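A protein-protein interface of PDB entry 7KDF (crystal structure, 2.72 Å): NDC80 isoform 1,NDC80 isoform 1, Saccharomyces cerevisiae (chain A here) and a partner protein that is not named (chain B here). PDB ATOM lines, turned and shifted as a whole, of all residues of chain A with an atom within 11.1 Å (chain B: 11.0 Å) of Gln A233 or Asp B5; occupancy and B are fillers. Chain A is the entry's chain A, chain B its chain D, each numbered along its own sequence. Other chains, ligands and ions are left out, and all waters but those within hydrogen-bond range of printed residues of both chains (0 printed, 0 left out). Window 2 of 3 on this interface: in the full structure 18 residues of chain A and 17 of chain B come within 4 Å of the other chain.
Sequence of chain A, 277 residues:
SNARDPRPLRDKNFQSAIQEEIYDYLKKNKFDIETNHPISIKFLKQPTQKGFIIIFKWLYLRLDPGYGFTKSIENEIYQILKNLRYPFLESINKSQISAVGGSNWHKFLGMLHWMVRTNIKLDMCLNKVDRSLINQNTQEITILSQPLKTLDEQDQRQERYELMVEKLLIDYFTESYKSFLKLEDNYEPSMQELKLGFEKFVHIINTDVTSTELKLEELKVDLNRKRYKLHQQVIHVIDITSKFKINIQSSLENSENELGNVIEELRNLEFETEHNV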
ATOM      1  N   ASN A 224       5.378 -13.833  19.295  1.00  0.00           N
ATOM      2  CA  ASN A 224       6.802 -14.157  19.314  1.00  0.00           C
ATOM      3  C   ASN A 224       7.021 -15.643  19.559  1.00  0.00           C
ATOM      4  O   ASN A 224       7.857 -16.273  18.901  1.00  0.00           O
ATOM      5  CB  ASN A 224       7.520 -13.338  20.387  1.00  0.00           C
ATOM      6  CG  ASN A 224       7.707 -11.884  19.994  1.00  0.00           C
ATOM      7  OD1 ASN A 224       7.564 -11.514  18.826  1.00  0.00           O
ATOM      8  ND2 ASN A 224       8.039 -11.050  20.973  1.00  0.00           N
ATOM      9  N   ARG A 225       6.273 -16.221  20.500  1.00  0.00           N
ATOM     10  CA  ARG A 225       6.413 -17.645  20.785  1.00  0.00           C
ATOM     11  C   ARG A 225       5.938 -18.493  19.611  1.00  0.00           C
ATOM     12  O   ARG A 225       6.596 -19.475  19.244  1.00  0.00           O
ATOM     13  CB  ARG A 225       5.633 -17.999  22.048  1.00  0.00           C
ATOM     14  CG  ARG A 225       6.104 -17.277  23.297  1.00  0.00           C
ATOM     15  CD  ARG A 225       5.249 -17.663  24.484  1.00  0.00           C
ATOM     16  NE  ARG A 225       5.718 -17.059  25.721  1.00  0.00           N
ATOM     17  CZ  ARG A 225       5.167 -17.286  26.907  1.00  0.00           C
ATOM     18  NH1 ARG A 225       4.131 -18.109  27.000  1.00  0.00           N
ATOM     19  NH2 ARG A 225       5.650 -16.700  27.995  1.00  0.00           N
ATOM     20  N   LYS A 226       4.799 -18.133  19.015  1.00  0.00           N
ATOM     21  CA  LYS A 226       4.269 -18.907  17.898  1.00  0.00           C
ATOM     22  C   LYS A 226       5.230 -18.893  16.718  1.00  0.00           C
ATOM     23  O   LYS A 226       5.459 -19.929  16.081  1.00  0.00           O
ATOM     24  CB  LYS A 226       2.904 -18.359  17.475  1.00  0.00           C
ATOM     25  CG  LYS A 226       1.749 -18.654  18.421  1.00  0.00           C
ATOM     26  CD  LYS A 226       0.444 -18.111  17.840  1.00  0.00           C
ATOM     27  CE  LYS A 226      -0.730 -18.253  18.799  1.00  0.00           C
ATOM     28  NZ  LYS A 226      -1.182 -19.661  18.968  1.00  0.00           N
ATOM     29  N   ARG A 227       5.803 -17.724  16.412  1.00  0.00           N
ATOM     30  CA  ARG A 227       6.736 -17.624  15.294  1.00  0.00           C
ATOM     31  C   ARG A 227       7.979 -18.467  15.535  1.00  0.00           C
ATOM     32  O   ARG A 227       8.454 -19.157  14.627  1.00  0.00           O
ATOM     33  CB  ARG A 227       7.124 -16.165  15.061  1.00  0.00           C
ATOM     34  CG  ARG A 227       8.321 -15.994  14.148  1.00  0.00           C
ATOM     35  CD  ARG A 227       8.650 -14.532  13.933  1.00  0.00           C
ATOM     36  NE  ARG A 227       7.496 -13.788  13.445  1.00  0.00           N
ATOM     37  CZ  ARG A 227       6.881 -12.835  14.136  1.00  0.00           C
ATOM     38  NH1 ARG A 227       7.313 -12.510  15.351  1.00  0.00           N
ATOM     39  NH2 ARG A 227       5.835 -12.208  13.614  1.00  0.00           N
ATOM     40  N   TYR A 228       8.522 -18.423  16.752  1.00  0.00           N
ATOM     41  CA  TYR A 228       9.686 -19.243  17.063  1.00  0.00           C
ATOM     42  C   TYR A 228       9.371 -20.721  16.883  1.00  0.00           C
ATOM     43  O   TYR A 228      10.169 -21.467  16.304  1.00  0.00           O
ATOM     44  CB  TYR A 228      10.169 -18.959  18.489  1.00  0.00           C
ATOM     45  CG  TYR A 228      11.325 -19.835  18.928  1.00  0.00           C
ATOM     46  CD1 TYR A 228      12.642 -19.443  18.707  1.00  0.00           C
ATOM     47  CD2 TYR A 228      11.100 -21.050  19.564  1.00  0.00           C
ATOM     48  CE1 TYR A 228      13.703 -20.242  19.104  1.00  0.00           C
ATOM     49  CE2 TYR A 228      12.150 -21.855  19.962  1.00  0.00           C
ATOM     50  CZ  TYR A 228      13.449 -21.448  19.733  1.00  0.00           C
ATOM     51  OH  TYR A 228      14.491 -22.253  20.135  1.00  0.00           O
ATOM     52  N   LYS A 229       8.204 -21.160  17.362  1.00  0.00           N
ATOM     53  CA  LYS A 229       7.824 -22.558  17.200  1.00  0.00           C
ATOM     54  C   LYS A 229       7.704 -22.920  15.726  1.00  0.00           C
ATOM     55  O   LYS A 229       8.149 -23.994  15.305  1.00  0.00           O
ATOM     56  CB  LYS A 229       6.511 -22.835  17.934  1.00  0.00           C
ATOM     57  CG  LYS A 229       6.709 -23.391  19.338  1.00  0.00           C
ATOM     58  CD  LYS A 229       5.481 -24.137  19.837  1.00  0.00           C
ATOM     59  CE  LYS A 229       5.657 -24.558  21.292  1.00  0.00           C
ATOM     60  NZ  LYS A 229       6.755 -25.553  21.460  1.00  0.00           N
ATOM     61  N   LEU A 230       7.114 -22.027  14.929  1.00  0.00           N
ATOM     62  CA  LEU A 230       6.966 -22.281  13.500  1.00  0.00           C
ATOM     63  C   LEU A 230       8.320 -22.391  12.812  1.00  0.00           C
ATOM     64  O   LEU A 230       8.526 -23.273  11.971  1.00  0.00           O
ATOM     65  CB  LEU A 230       6.127 -21.176  12.859  1.00  0.00           C
ATOM     66  CG  LEU A 230       5.802 -21.320  11.375  1.00  0.00           C
ATOM     67  CD1 LEU A 230       5.074 -22.630  11.120  1.00  0.00           C
ATOM     68  CD2 LEU A 230       4.971 -20.136  10.907  1.00  0.00           C
ATOM     69  N   HIS A 231       9.257 -21.503  13.154  1.00  0.00           N
ATOM     70  CA  HIS A 231      10.584 -21.576  12.552  1.00  0.00           C
ATOM     71  C   HIS A 231      11.277 -22.888  12.901  1.00  0.00           C
ATOM     72  O   HIS A 231      11.889 -23.519  12.033  1.00  0.00           O
ATOM     73  CB  HIS A 231      11.431 -20.382  12.990  1.00  0.00           C
ATOM     74  CG  HIS A 231      11.119 -19.120  12.249  1.00  0.00           C
ATOM     75  ND1 HIS A 231      12.036 -18.107  12.085  1.00  0.00           N
ATOM     76  CD2 HIS A 231       9.987 -18.707  11.628  1.00  0.00           C
ATOM     77  CE1 HIS A 231      11.487 -17.123  11.394  1.00  0.00           C
ATOM     78  NE2 HIS A 231      10.242 -17.461  11.107  1.00  0.00           N
ATOM     79  N   GLN A 232      11.181 -23.321  14.161  1.00  0.00           N
ATOM     80  CA  GLN A 232      11.727 -24.621  14.541  1.00  0.00           C
ATOM     81  C   GLN A 232      11.105 -25.739  13.715  1.00  0.00           C
ATOM     82  O   GLN A 232      11.788 -26.700  13.341  1.00  0.00           O
ATOM     83  CB  GLN A 232      11.497 -24.874  16.031  1.00  0.00           C
ATOM     84  CG  GLN A 232      12.194 -23.887  16.944  1.00  0.00           C
ATOM     85  CD  GLN A 232      13.699 -23.953  16.826  1.00  0.00           C
ATOM     86  OE1 GLN A 232      14.325 -24.914  17.273  1.00  0.00           O
ATOM     87  NE2 GLN A 232      14.293 -22.926  16.228  1.00  0.00           N
ATOM     88  N   GLN A 233       9.806 -25.633  13.426  1.00  0.00           N
ATOM     89  CA  GLN A 233       9.157 -26.607  12.555  1.00  0.00           C
ATOM     90  C   GLN A 233       9.794 -26.601  11.171  1.00  0.00           C
ATOM     91  O   GLN A 233      10.055 -27.663  10.590  1.00  0.00           O
ATOM     92  CB  GLN A 233       7.668 -26.292  12.448  1.00  0.00           C
ATOM     93  CG  GLN A 233       6.773 -27.035  13.421  1.00  0.00           C
ATOM     94  CD  GLN A 233       5.310 -26.672  13.220  1.00  0.00           C
ATOM     95  OE1 GLN A 233       4.897 -25.544  13.494  1.00  0.00           O
ATOM     96  NE2 GLN A 233       4.522 -27.626  12.740  1.00  0.00           N
ATOM     97  N   VAL A 234      10.061 -25.407  10.635  1.00  0.00           N
ATOM     98  CA  VAL A 234      10.733 -25.296   9.343  1.00  0.00           C
ATOM     99  C   VAL A 234      12.128 -25.905   9.417  1.00  0.00           C
ATOM    100  O   VAL A 234      12.563 -26.605   8.496  1.00  0.00           O
ATOM    101  CB  VAL A 234      10.779 -23.826   8.884  1.00  0.00           C
ATOM    102  CG1 VAL A 234      11.658 -23.675   7.653  1.00  0.00           C
ATOM    103  CG2 VAL A 234       9.379 -23.321   8.603  1.00  0.00           C
ATOM    104  N   ILE A 235      12.847 -25.661  10.515  1.00  0.00           N
ATOM    105  CA  ILE A 235      14.181 -26.235  10.667  1.00  0.00           C
ATOM    106  C   ILE A 235      14.106 -27.752  10.581  1.00  0.00           C
ATOM    107  O   ILE A 235      14.906 -28.396   9.890  1.00  0.00           O
ATOM    108  CB  ILE A 235      14.809 -25.806  12.004  1.00  0.00           C
ATOM    109  CG1 ILE A 235      14.841 -24.287  12.140  1.00  0.00           C
ATOM    110  CG2 ILE A 235      16.247 -26.312  12.083  1.00  0.00           C
ATOM    111  CD1 ILE A 235      15.632 -23.607  11.099  1.00  0.00           C
ATOM    112  N   HIS A 236      13.128 -28.340  11.275  1.00  0.00           N
ATOM    113  CA  HIS A 236      12.967 -29.789  11.296  1.00  0.00           C
ATOM    114  C   HIS A 236      12.688 -30.344   9.904  1.00  0.00           C
ATOM    115  O   HIS A 236      13.228 -31.389   9.521  1.00  0.00           O
ATOM    116  CB  HIS A 236      11.840 -30.155  12.258  1.00  0.00           C
ATOM    117  CG  HIS A 236      11.698 -31.626  12.493  1.00  0.00           C
ATOM    118  ND1 HIS A 236      12.737 -32.414  12.944  1.00  0.00           N
ATOM    119  CD2 HIS A 236      10.636 -32.453  12.349  1.00  0.00           C
ATOM    120  CE1 HIS A 236      12.321 -33.662  13.064  1.00  0.00           C
ATOM    121  NE2 HIS A 236      11.050 -33.713  12.710  1.00  0.00           N
ATOM    122  N   VAL A 237      11.830 -29.665   9.140  1.00  0.00           N
ATOM    123  CA  VAL A 237      11.514 -30.113   7.787  1.00  0.00           C
ATOM    124  C   VAL A 237      12.768 -30.098   6.926  1.00  0.00           C
ATOM    125  O   VAL A 237      13.083 -31.070   6.231  1.00  0.00           O
ATOM    126  CB  VAL A 237      10.410 -29.229   7.179  1.00  0.00           C
ATOM    127  CG1 VAL A 237      10.411 -29.342   5.659  1.00  0.00           C
ATOM    128  CG2 VAL A 237       9.055 -29.587   7.764  1.00  0.00           C
ATOM    129  N   ILE A 238      13.516 -28.998   6.983  1.00  0.00           N
ATOM    130  CA  ILE A 238      14.726 -28.868   6.184  1.00  0.00           C
ATOM    131  C   ILE A 238      15.798 -29.837   6.658  1.00  0.00           C
ATOM    132  O   ILE A 238      16.553 -30.392   5.850  1.00  0.00           O
ATOM    133  CB  ILE A 238      15.203 -27.410   6.222  1.00  0.00           C
ATOM    134  CG1 ILE A 238      14.068 -26.535   5.701  1.00  0.00           C
ATOM    135  CG2 ILE A 238      16.485 -27.239   5.421  1.00  0.00           C
ATOM    136  CD1 ILE A 238      14.406 -25.133   5.504  1.00  0.00           C
ATOM    137  N   ASP A 239      15.888 -30.060   7.971  1.00  0.00           N
ATOM    138  CA  ASP A 239      16.930 -30.937   8.493  1.00  0.00           C
ATOM    139  C   ASP A 239      16.767 -32.362   7.990  1.00  0.00           C
ATOM    140  O   ASP A 239      17.748 -32.999   7.588  1.00  0.00           O
ATOM    141  CB  ASP A 239      16.936 -30.916  10.020  1.00  0.00           C
ATOM    142  CG  ASP A 239      17.770 -32.038  10.611  1.00  0.00           C
ATOM    143  OD1 ASP A 239      19.013 -31.979  10.511  1.00  0.00           O
ATOM    144  OD2 ASP A 239      17.182 -32.984  11.174  1.00  0.00           O
ATOM    145  N   ILE A 240      15.543 -32.891   7.999  1.00  0.00           N
ATOM    146  CA  ILE A 240      15.388 -34.296   7.651  1.00  0.00           C
ATOM    147  C   ILE A 240      15.062 -34.500   6.176  1.00  0.00           C
ATOM    148  O   ILE A 240      15.279 -35.604   5.658  1.00  0.00           O
ATOM    149  CB  ILE A 240      14.327 -35.006   8.514  1.00  0.00           C
ATOM    150  CG1 ILE A 240      12.931 -34.647   8.054  1.00  0.00           C
ATOM    151  CG2 ILE A 240      14.473 -34.621   9.987  1.00  0.00           C
ATOM    152  CD1 ILE A 240      11.927 -35.596   8.595  1.00  0.00           C
ATOM    153  N   THR A 241      14.538 -33.481   5.488  1.00  0.00           N
ATOM    154  CA  THR A 241      14.414 -33.585   4.036  1.00  0.00           C
ATOM    155  C   THR A 241      15.787 -33.699   3.393  1.00  0.00           C
ATOM    156  O   THR A 241      16.018 -34.561   2.538  1.00  0.00           O
ATOM    157  CB  THR A 241      13.652 -32.384   3.468  1.00  0.00           C
ATOM    158  OG1 THR A 241      12.265 -32.492   3.804  1.00  0.00           O
ATOM    159  CG2 THR A 241      13.792 -32.329   1.951  1.00  0.00           C
ATOM    160  N   SER A 242      16.719 -32.841   3.809  1.00  0.00           N
ATOM    161  CA  SER A 242      18.075 -32.912   3.278  1.00  0.00           C
ATOM    162  C   SER A 242      18.755 -34.216   3.675  1.00  0.00           C
ATOM    163  O   SER A 242      19.422 -34.852   2.851  1.00  0.00           O
ATOM    164  CB  SER A 242      18.888 -31.711   3.757  1.00  0.00           C
ATOM    165  OG  SER A 242      19.019 -31.725   5.165  1.00  0.00           O
ATOM    166  N   ALA B   2      -2.181 -29.888   2.795  1.00  0.00           N
ATOM    167  CA  ALA B   2      -0.766 -29.990   3.136  1.00  0.00           C
ATOM    168  C   ALA B   2      -0.362 -28.909   4.137  1.00  0.00           C
ATOM    169  O   ALA B   2       0.044 -27.809   3.755  1.00  0.00           O
ATOM    170  CB  ALA B   2       0.091 -29.899   1.880  1.00  0.00           C
ATOM    171  N   SER B   3      -0.480 -29.228   5.421  1.00  0.00           N
ATOM    172  CA  SER B   3      -0.073 -28.331   6.493  1.00  0.00           C
ATOM    173  C   SER B   3       1.223 -28.826   7.116  1.00  0.00           C
ATOM    174  O   SER B   3       1.388 -30.026   7.356  1.00  0.00           O
ATOM    175  CB  SER B   3      -1.155 -28.218   7.570  1.00  0.00           C
ATOM    176  OG  SER B   3      -0.855 -27.160   8.465  1.00  0.00           O
ATOM    177  N   ILE B   4       2.138 -27.889   7.379  1.00  0.00           N
ATOM    178  CA  ILE B   4       3.424 -28.236   7.972  1.00  0.00           C
ATOM    179  C   ILE B   4       3.259 -28.885   9.342  1.00  0.00           C
ATOM    180  O   ILE B   4       4.149 -29.615   9.791  1.00  0.00           O
ATOM    181  CB  ILE B   4       4.332 -26.985   8.037  1.00  0.00           C
ATOM    182  CG1 ILE B   4       5.747 -27.346   8.503  1.00  0.00           C
ATOM    183  CG2 ILE B   4       3.717 -25.898   8.890  1.00  0.00           C
ATOM    184  CD1 ILE B   4       6.751 -26.228   8.342  1.00  0.00           C
ATOM    185  N   ASP B   5       2.132 -28.651  10.020  1.00  0.00           N
ATOM    186  CA  ASP B   5       1.861 -29.392  11.246  1.00  0.00           C
ATOM    187  C   ASP B   5       1.683 -30.878  10.977  1.00  0.00           C
ATOM    188  O   ASP B   5       1.902 -31.693  11.878  1.00  0.00           O
ATOM    189  CB  ASP B   5       0.622 -28.832  11.948  1.00  0.00           C
ATOM    190  CG  ASP B   5       0.761 -27.361  12.289  1.00  0.00           C
ATOM    191  OD1 ASP B   5       1.767 -26.992  12.928  1.00  0.00           O
ATOM    192  OD2 ASP B   5      -0.136 -26.575  11.916  1.00  0.00           O
ATOM    193  N   ALA B   6       1.307 -31.247   9.750  1.00  0.00           N
ATOM    194  CA  ALA B   6       1.145 -32.637   9.352  1.00  0.00           C
ATOM    195  C   ALA B   6       2.425 -33.230   8.772  1.00  0.00           C
ATOM    196  O   ALA B   6       2.372 -34.276   8.114  1.00  0.00           O
ATOM    197  CB  ALA B   6       0.002 -32.764   8.344  1.00  0.00           C
ATOM    198  N   PHE B   7       3.570 -32.586   9.009  1.00  0.00           N
ATOM    199  CA  PHE B   7       4.825 -33.059   8.436  1.00  0.00           C
ATOM    200  C   PHE B   7       5.214 -34.433   8.965  1.00  0.00           C
ATOM    201  O   PHE B   7       5.914 -35.185   8.277  1.00  0.00           O
ATOM    202  CB  PHE B   7       5.936 -32.052   8.719  1.00  0.00           C
ATOM    203  CG  PHE B   7       7.286 -32.503   8.265  1.00  0.00           C
ATOM    204  CD1 PHE B   7       7.550 -32.690   6.915  1.00  0.00           C
ATOM    205  CD2 PHE B   7       8.290 -32.749   9.184  1.00  0.00           C
ATOM    206  CE1 PHE B   7       8.793 -33.106   6.492  1.00  0.00           C
ATOM    207  CE2 PHE B   7       9.535 -33.165   8.767  1.00  0.00           C
ATOM    208  CZ  PHE B   7       9.783 -33.342   7.417  1.00  0.00           C
ATOM    209  N   SER B   8       4.779 -34.779  10.176  1.00  0.00           N
ATOM    210  CA  SER B   8       5.104 -36.087  10.732  1.00  0.00           C
ATOM    211  C   SER B   8       4.485 -37.224   9.930  1.00  0.00           C
ATOM    212  O   SER B   8       5.005 -38.344   9.968  1.00  0.00           O
ATOM    213  CB  SER B   8       4.650 -36.165  12.190  1.00  0.00           C
ATOM    214  OG  SER B   8       3.351 -35.621  12.341  1.00  0.00           O
ATOM    215  N   ASP B   9       3.390 -36.967   9.211  1.00  0.00           N
ATOM    216  CA  ASP B   9       2.814 -37.991   8.345  1.00  0.00           C
ATOM    217  C   ASP B   9       3.741 -38.295   7.175  1.00  0.00           C
ATOM    218  O   ASP B   9       4.028 -39.460   6.878  1.00  0.00           O
ATOM    219  CB  ASP B   9       1.443 -37.540   7.841  1.00  0.00           C
ATOM    220  CG  ASP B   9       0.399 -37.492   8.941  1.00  0.00           C
ATOM    221  OD1 ASP B   9       0.705 -37.918  10.076  1.00  0.00           O
ATOM    222  OD2 ASP B   9      -0.729 -37.025   8.670  1.00  0.00           O
ATOM    223  N   LEU B  10       4.214 -37.247   6.498  1.00  0.00           N
ATOM    224  CA  LEU B  10       5.193 -37.409   5.431  1.00  0.00           C
ATOM    225  C   LEU B  10       6.541 -37.892   5.956  1.00  0.00           C
ATOM    226  O   LEU B  10       7.228 -38.659   5.271  1.00  0.00           O
ATOM    227  CB  LEU B  10       5.306 -36.090   4.659  1.00  0.00           C
ATOM    228  CG  LEU B  10       6.256 -35.909   3.483  1.00  0.00           C
ATOM    229  CD1 LEU B  10       5.680 -34.986   2.438  1.00  0.00           C
ATOM    230  CD2 LEU B  10       7.446 -35.213   4.082  1.00  0.00           C
ATOM    231  N   GLU B  11       6.930 -37.476   7.163  1.00  0.00           N
ATOM    232  CA  GLU B  11       8.160 -37.992   7.756  1.00  0.00           C
ATOM    233  C   GLU B  11       8.098 -39.505   7.913  1.00  0.00           C
ATOM    234  O   GLU B  11       9.092 -40.203   7.677  1.00  0.00           O
ATOM    235  CB  GLU B  11       8.416 -37.316   9.103  1.00  0.00           C
ATOM    236  CG  GLU B  11       9.600 -37.877   9.878  1.00  0.00           C
ATOM    237  CD  GLU B  11      10.078 -36.934  10.971  1.00  0.00           C
ATOM    238  OE1 GLU B  11       9.298 -36.046  11.376  1.00  0.00           O
ATOM    239  OE2 GLU B  11      11.240 -37.068  11.413  1.00  0.00           O
ATOM    240  N   ARG B  12       6.939 -40.032   8.318  1.00  0.00           N
ATOM    241  CA  ARG B  12       6.784 -41.479   8.437  1.00  0.00           C
ATOM    242  C   ARG B  12       6.931 -42.163   7.084  1.00  0.00           C
ATOM    243  O   ARG B  12       7.583 -43.209   6.979  1.00  0.00           O
ATOM    244  CB  ARG B  12       5.427 -41.815   9.057  1.00  0.00           C
ATOM    245  CG  ARG B  12       5.489 -42.226  10.519  1.00  0.00           C
ATOM    246  CD  ARG B  12       4.183 -42.870  10.965  1.00  0.00           C
ATOM    247  NE  ARG B  12       3.144 -41.877  11.227  1.00  0.00           N
ATOM    248  CZ  ARG B  12       2.191 -41.544  10.361  1.00  0.00           C
ATOM    249  NH1 ARG B  12       2.137 -42.127   9.170  1.00  0.00           N
ATOM    250  NH2 ARG B  12       1.287 -40.628  10.686  1.00  0.00           N
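The side-chain amide nitrogen (NE2) of Gln A233 sits at hydrogen-bond distance from the side-chain carboxylate (OD1) of Asp B5 (2.8 Å). OE1 of Glu B11 sits at hydrogen-bond distance from NE2 of His A236 (3.2 Å).
O of Val A237 lies within hydrogen-bond range of OG1 of Thr A241 (2.9 Å).
Among the printed residues, pairs that only touch across the chains: Ile A240 with Glu B11, Ile A240 with Phe B7, Val A237 with Phe B7, Gln A233 with Ile B4, His A236 with Phe B7 and Val A234 with Ile B4.
No residue of chain B comes within 4 Å of Leu A230. No residue of chain B comes within 4 Å of Gln A232. Gln A233 touches just these residues of chain B: Ile B4 (3.6 Å) and Asp B5 (2.8 Å). Val A234 touches just one residue of chain B: Ile B4 (3.9 Å). No residue of chain B comes within 4 Å of Ile A235. Of the printed residues of chain B, His A236 touches Phe B7 (3.8 Å) and Glu B11 (3.2 Å). Of the printed residues of chain B, Val A237 touches Phe B7 (3.4 Å). Printed residues of chain B within 4 Å of Ile A240: Phe B7 (3.3 Å) and Glu B11 (3.3 Å). No residue of chain A comes within 4 Å of Ser B3. Ile B4 touches just these residues of chain A: Gln A233 (3.6 Å) and Val A234 (3.9 Å). Asp B5 touches one residue of chain A. No residue of chain A comes within 4 Å of Ala B6. Printed residues of chain A within 4 Å of Glu B11: His A236 (3.2 Å) and Ile A240 (3.3 Å). The nearest residue of chain A that does not touch Asp B5 is Leu A230 (5.8 Å). The nearest printed residue of chain A that does not touch Glu B11 is Asp A239 (7.2 Å).
Of the 11 printed residues of chain B, 4 touch a printed residue of chain A.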
